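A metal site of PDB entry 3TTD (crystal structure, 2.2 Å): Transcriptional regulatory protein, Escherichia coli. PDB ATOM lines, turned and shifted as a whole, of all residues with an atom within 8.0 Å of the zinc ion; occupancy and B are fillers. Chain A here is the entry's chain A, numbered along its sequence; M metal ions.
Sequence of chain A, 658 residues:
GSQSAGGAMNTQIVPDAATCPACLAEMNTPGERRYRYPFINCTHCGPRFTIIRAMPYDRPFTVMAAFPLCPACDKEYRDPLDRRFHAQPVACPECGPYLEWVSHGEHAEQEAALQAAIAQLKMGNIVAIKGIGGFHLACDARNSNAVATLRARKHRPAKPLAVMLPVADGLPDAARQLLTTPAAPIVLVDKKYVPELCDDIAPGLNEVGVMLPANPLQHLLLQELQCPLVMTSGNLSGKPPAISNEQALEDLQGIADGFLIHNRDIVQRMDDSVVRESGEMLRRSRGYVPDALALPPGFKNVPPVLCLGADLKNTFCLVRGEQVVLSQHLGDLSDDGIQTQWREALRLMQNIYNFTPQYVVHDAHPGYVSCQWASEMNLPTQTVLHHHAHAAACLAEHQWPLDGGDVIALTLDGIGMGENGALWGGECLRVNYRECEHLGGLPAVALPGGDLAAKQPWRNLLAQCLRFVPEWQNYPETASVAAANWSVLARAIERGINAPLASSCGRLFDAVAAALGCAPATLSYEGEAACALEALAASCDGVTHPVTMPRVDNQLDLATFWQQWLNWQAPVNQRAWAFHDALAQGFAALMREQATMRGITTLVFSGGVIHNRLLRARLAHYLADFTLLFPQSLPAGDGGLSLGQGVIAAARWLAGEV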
ATOM      1  N   ALA A  17      20.970  13.680 -11.627  1.00  0.00           N
ATOM      2  CA  ALA A  17      19.896  14.484 -12.234  1.00  0.00           C
ATOM      3  C   ALA A  17      20.333  15.368 -13.392  1.00  0.00           C
ATOM      4  O   ALA A  17      21.371  15.993 -13.330  1.00  0.00           O
ATOM      5  CB  ALA A  17      19.098  15.320 -11.181  1.00  0.00           C
ATOM      6  N   ALA A  18      19.516  15.402 -14.453  1.00  0.00           N
ATOM      7  CA  ALA A  18      19.763  16.234 -15.627  1.00  0.00           C
ATOM      8  C   ALA A  18      19.991  17.675 -15.194  1.00  0.00           C
ATOM      9  O   ALA A  18      19.250  18.168 -14.365  1.00  0.00           O
ATOM     10  CB  ALA A  18      18.556  16.172 -16.572  1.00  0.00           C
ATOM     11  N   THR A  19      20.965  18.367 -15.781  1.00  0.00           N
ATOM     12  CA  THR A  19      21.101  19.832 -15.647  1.00  0.00           C
ATOM     13  C   THR A  19      19.722  20.530 -15.705  1.00  0.00           C
ATOM     14  O   THR A  19      18.938  20.270 -16.641  1.00  0.00           O
ATOM     15  CB  THR A  19      22.047  20.323 -16.790  1.00  0.00           C
ATOM     16  OG1 THR A  19      23.238  19.522 -16.737  1.00  0.00           O
ATOM     17  CG2 THR A  19      22.428  21.834 -16.665  1.00  0.00           C
ATOM     18  N   CYS A  20      19.402  21.396 -14.709  1.00  0.00           N
ATOM     19  CA  CYS A  20      18.074  22.055 -14.627  1.00  0.00           C
ATOM     20  C   CYS A  20      17.969  23.303 -15.524  1.00  0.00           C
ATOM     21  O   CYS A  20      18.976  23.766 -16.049  1.00  0.00           O
ATOM     22  CB  CYS A  20      17.750  22.410 -13.173  1.00  0.00           C
ATOM     23  SG  CYS A  20      18.793  23.773 -12.476  1.00  0.00           S
ATOM     24  N   PRO A  21      16.745  23.828 -15.738  1.00  0.00           N
ATOM     25  CA  PRO A  21      16.635  25.038 -16.601  1.00  0.00           C
ATOM     26  C   PRO A  21      17.486  26.238 -16.137  1.00  0.00           C
ATOM     27  O   PRO A  21      18.176  26.851 -16.938  1.00  0.00           O
ATOM     28  CB  PRO A  21      15.141  25.370 -16.567  1.00  0.00           C
ATOM     29  CG  PRO A  21      14.492  23.980 -16.378  1.00  0.00           C
ATOM     30  CD  PRO A  21      15.420  23.321 -15.347  1.00  0.00           C
ATOM     31  N   ALA A  22      17.496  26.501 -14.841  1.00  0.00           N
ATOM     32  CA  ALA A  22      18.296  27.591 -14.247  1.00  0.00           C
ATOM     33  C   ALA A  22      19.817  27.466 -14.422  1.00  0.00           C
ATOM     34  O   ALA A  22      20.482  28.471 -14.620  1.00  0.00           O
ATOM     35  CB  ALA A  22      17.925  27.743 -12.752  1.00  0.00           C
ATOM     36  N   CYS A  23      20.388  26.274 -14.340  1.00  0.00           N
ATOM     37  CA  CYS A  23      21.835  26.081 -14.537  1.00  0.00           C
ATOM     38  C   CYS A  23      22.134  26.203 -16.032  1.00  0.00           C
ATOM     39  O   CYS A  23      23.125  26.814 -16.452  1.00  0.00           O
ATOM     40  CB  CYS A  23      22.315  24.723 -14.023  1.00  0.00           C
ATOM     41  SG  CYS A  23      22.552  24.584 -12.196  1.00  0.00           S
ATOM     42  N   LEU A  24      21.253  25.626 -16.840  1.00  0.00           N
ATOM     43  CA  LEU A  24      21.349  25.798 -18.289  1.00  0.00           C
ATOM     44  C   LEU A  24      21.327  27.295 -18.740  1.00  0.00           C
ATOM     45  O   LEU A  24      22.159  27.699 -19.550  1.00  0.00           O
ATOM     46  CB  LEU A  24      20.305  24.930 -18.983  1.00  0.00           C
ATOM     47  CG  LEU A  24      20.452  24.920 -20.488  1.00  0.00           C
ATOM     48  CD1 LEU A  24      21.844  24.341 -20.882  1.00  0.00           C
ATOM     49  CD2 LEU A  24      19.252  24.201 -21.167  1.00  0.00           C
ATOM     50  N   GLU A  26      22.152  29.891 -16.730  1.00  0.00           N
ATOM     51  CA  GLU A  26      23.397  30.463 -16.191  1.00  0.00           C
ATOM     52  C   GLU A  26      24.559  30.163 -17.127  1.00  0.00           C
ATOM     53  O   GLU A  26      25.324  31.059 -17.468  1.00  0.00           O
ATOM     54  CB  GLU A  26      23.665  29.938 -14.772  1.00  0.00           C
ATOM     55  CG  GLU A  26      24.921  30.460 -14.074  1.00  0.00           C
ATOM     56  CD  GLU A  26      25.060  29.915 -12.632  1.00  0.00           C
ATOM     57  OE1 GLU A  26      24.052  29.393 -12.073  1.00  0.00           O
ATOM     58  OE2 GLU A  26      26.196  30.018 -12.080  1.00  0.00           O
ATOM     59  N   ILE A  40      28.844  23.018 -14.325  1.00  0.00           N
ATOM     60  CA  ILE A  40      27.835  23.730 -13.574  1.00  0.00           C
ATOM     61  C   ILE A  40      26.799  22.732 -12.995  1.00  0.00           C
ATOM     62  O   ILE A  40      26.311  21.819 -13.703  1.00  0.00           O
ATOM     63  CB  ILE A  40      27.150  24.820 -14.469  1.00  0.00           C
ATOM     64  CG1 ILE A  40      26.155  25.687 -13.679  1.00  0.00           C
ATOM     65  CG2 ILE A  40      26.447  24.208 -15.671  1.00  0.00           C
ATOM     66  CD1 ILE A  40      25.852  27.013 -14.435  1.00  0.00           C
ATOM     67  N   ASN A  41      26.478  22.905 -11.707  1.00  0.00           N
ATOM     68  CA  ASN A  41      25.371  22.164 -11.085  1.00  0.00           C
ATOM     69  C   ASN A  41      24.825  22.983  -9.935  1.00  0.00           C
ATOM     70  O   ASN A  41      25.443  23.962  -9.535  1.00  0.00           O
ATOM     71  CB  ASN A  41      25.788  20.755 -10.609  1.00  0.00           C
ATOM     72  CG  ASN A  41      26.982  20.781  -9.647  1.00  0.00           C
ATOM     73  OD1 ASN A  41      28.107  20.529 -10.053  1.00  0.00           O
ATOM     74  ND2 ASN A  41      26.755  21.124  -8.400  1.00  0.00           N
ATOM     75  N   CYS A  42      23.672  22.604  -9.411  1.00  0.00           N
ATOM     76  CA  CYS A  42      23.172  23.272  -8.217  1.00  0.00           C
ATOM     77  C   CYS A  42      22.542  22.268  -7.270  1.00  0.00           C
ATOM     78  O   CYS A  42      22.727  21.049  -7.412  1.00  0.00           O
ATOM     79  CB  CYS A  42      22.200  24.415  -8.593  1.00  0.00           C
ATOM     80  SG  CYS A  42      20.642  23.834  -9.224  1.00  0.00           S
ATOM     81  N   THR A  43      21.820  22.741  -6.285  1.00  0.00           N
ATOM     82  CA  THR A  43      21.194  21.841  -5.317  1.00  0.00           C
ATOM     83  C   THR A  43      20.139  20.919  -5.952  1.00  0.00           C
ATOM     84  O   THR A  43      19.881  19.831  -5.441  1.00  0.00           O
ATOM     85  CB  THR A  43      20.658  22.616  -4.064  1.00  0.00           C
ATOM     86  OG1 THR A  43      20.435  21.696  -2.988  1.00  0.00           O
ATOM     87  CG2 THR A  43      19.394  23.389  -4.368  1.00  0.00           C
ATOM     88  N   HIS A  44      19.607  21.323  -7.104  1.00  0.00           N
ATOM     89  CA  HIS A  44      18.548  20.590  -7.812  1.00  0.00           C
ATOM     90  C   HIS A  44      18.994  19.652  -8.940  1.00  0.00           C
ATOM     91  O   HIS A  44      18.141  18.958  -9.510  1.00  0.00           O
ATOM     92  CB  HIS A  44      17.488  21.564  -8.336  1.00  0.00           C
ATOM     93  CG  HIS A  44      16.846  22.346  -7.254  1.00  0.00           C
ATOM     94  ND1 HIS A  44      16.968  23.719  -7.148  1.00  0.00           N
ATOM     95  CD2 HIS A  44      16.151  21.938  -6.155  1.00  0.00           C
ATOM     96  CE1 HIS A  44      16.340  24.128  -6.063  1.00  0.00           C
ATOM     97  NE2 HIS A  44      15.837  23.066  -5.433  1.00  0.00           N
ATOM     98  N   CYS A  45      20.278  19.637  -9.284  1.00  0.00           N
ATOM     99  CA  CYS A  45      20.736  18.908 -10.460  1.00  0.00           C
ATOM    100  C   CYS A  45      22.220  18.549 -10.369  1.00  0.00           C
ATOM    101  O   CYS A  45      22.964  19.099  -9.524  1.00  0.00           O
ATOM    102  CB  CYS A  45      20.478  19.699 -11.762  1.00  0.00           C
ATOM    103  SG  CYS A  45      21.698  20.982 -12.147  1.00  0.00           S
ATOM    104  N   GLY A  46      22.647  17.639 -11.249  1.00  0.00           N
ATOM    105  CA  GLY A  46      24.016  17.269 -11.337  1.00  0.00           C
ATOM    106  C   GLY A  46      24.227  15.861 -10.792  1.00  0.00           C
ATOM    107  O   GLY A  46      23.285  15.209 -10.362  1.00  0.00           O
ATOM    108  N   ARG A  48      25.179  12.645  -8.530  1.00  0.00           N
ATOM    109  CA  ARG A  48      24.992  12.328  -7.097  1.00  0.00           C
ATOM    110  C   ARG A  48      25.691  10.996  -6.766  1.00  0.00           C
ATOM    111  O   ARG A  48      26.862  10.962  -6.383  1.00  0.00           O
ATOM    112  CB  ARG A  48      23.480  12.272  -6.741  1.00  0.00           C
ATOM    113  CG  ARG A  48      22.724  13.597  -6.839  1.00  0.00           C
ATOM    114  CD  ARG A  48      23.217  14.603  -5.794  1.00  0.00           C
ATOM    115  NE  ARG A  48      22.488  15.859  -5.916  1.00  0.00           N
ATOM    116  CZ  ARG A  48      22.870  16.910  -6.634  1.00  0.00           C
ATOM    117  NH1 ARG A  48      22.063  17.946  -6.647  1.00  0.00           N
ATOM    118  NH2 ARG A  48      24.012  16.933  -7.352  1.00  0.00           N
ATOM    119  N   ARG A  83      20.589  29.176  -4.871  1.00  0.00           N
ATOM    120  CA  ARG A  83      20.275  27.897  -5.549  1.00  0.00           C
ATOM    121  C   ARG A  83      21.368  26.833  -5.356  1.00  0.00           C
ATOM    122  O   ARG A  83      21.103  25.623  -5.399  1.00  0.00           O
ATOM    123  CB  ARG A  83      20.047  28.148  -7.041  1.00  0.00           C
ATOM    124  CG  ARG A  83      19.352  26.982  -7.758  1.00  0.00           C
ATOM    125  CD  ARG A  83      19.065  27.292  -9.214  1.00  0.00           C
ATOM    126  NE  ARG A  83      20.205  27.115 -10.096  1.00  0.00           N
ATOM    127  CZ  ARG A  83      20.987  28.087 -10.575  1.00  0.00           C
ATOM    128  NH1 ARG A  83      20.798  29.346 -10.235  1.00  0.00           N
ATOM    129  NH2 ARG A  83      21.984  27.806 -11.384  1.00  0.00           N
ATOM    130  N   ARG A  84      22.588  27.307  -5.145  1.00  0.00           N
ATOM    131  CA  ARG A  84      23.755  26.438  -5.005  1.00  0.00           C
ATOM    132  C   ARG A  84      24.095  26.148  -3.541  1.00  0.00           C
ATOM    133  O   ARG A  84      25.173  25.581  -3.251  1.00  0.00           O
ATOM    134  CB  ARG A  84      24.953  27.044  -5.745  1.00  0.00           C
ATOM    135  CG  ARG A  84      24.911  26.769  -7.235  1.00  0.00           C
ATOM    136  CD  ARG A  84      25.517  27.882  -8.072  1.00  0.00           C
ATOM    137  NE  ARG A  84      24.526  28.855  -8.540  1.00  0.00           N
ATOM    138  CZ  ARG A  84      24.406  30.118  -8.098  1.00  0.00           C
ATOM    139  NH1 ARG A  84      25.211  30.602  -7.149  1.00  0.00           N
ATOM    140  NH2 ARG A  84      23.481  30.920  -8.595  1.00  0.00           N
ATOM    141  N   ALA A  87      25.419  22.836  -2.500  1.00  0.00           N
ATOM    142  CA  ALA A  87      25.562  22.041  -3.713  1.00  0.00           C
ATOM    143  C   ALA A  87      26.941  21.378  -3.600  1.00  0.00           C
ATOM    144  O   ALA A  87      27.952  21.984  -3.919  1.00  0.00           O
ATOM    145  CB  ALA A  87      25.433  22.907  -4.995  1.00  0.00           C
HETATM  146 ZN    ZN M   1      20.898  23.191 -11.501  1.00  0.00          ZN
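The side-chain sulfur (SG) of Cys 42 sits close to the guanidinium group (NE) of Arg 83.
The guanidinium group of Arg 48 sits at hydrogen-bond distance from the backbone carbonyl oxygen of Cys 45 (3.2 Å).
SG of Cys 23 sits close to NH2 of Arg 83 (3.4 Å).
SG of Cys 42 sits close to N of His 44, 3.4 Å away.
NH1 of Arg 48 is in hydrogen-bond range of O of Cys 42.
Four residues have an atom within 4 Å of the zinc ion: Cys 20, Cys 23, Cys 42 and Cys 45.
The zinc ion is bound by SG of Cys 23, SG of Cys 42, SG of Cys 20 and SG of Cys 45.
The zinc ion has four donor atoms within binding distance.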
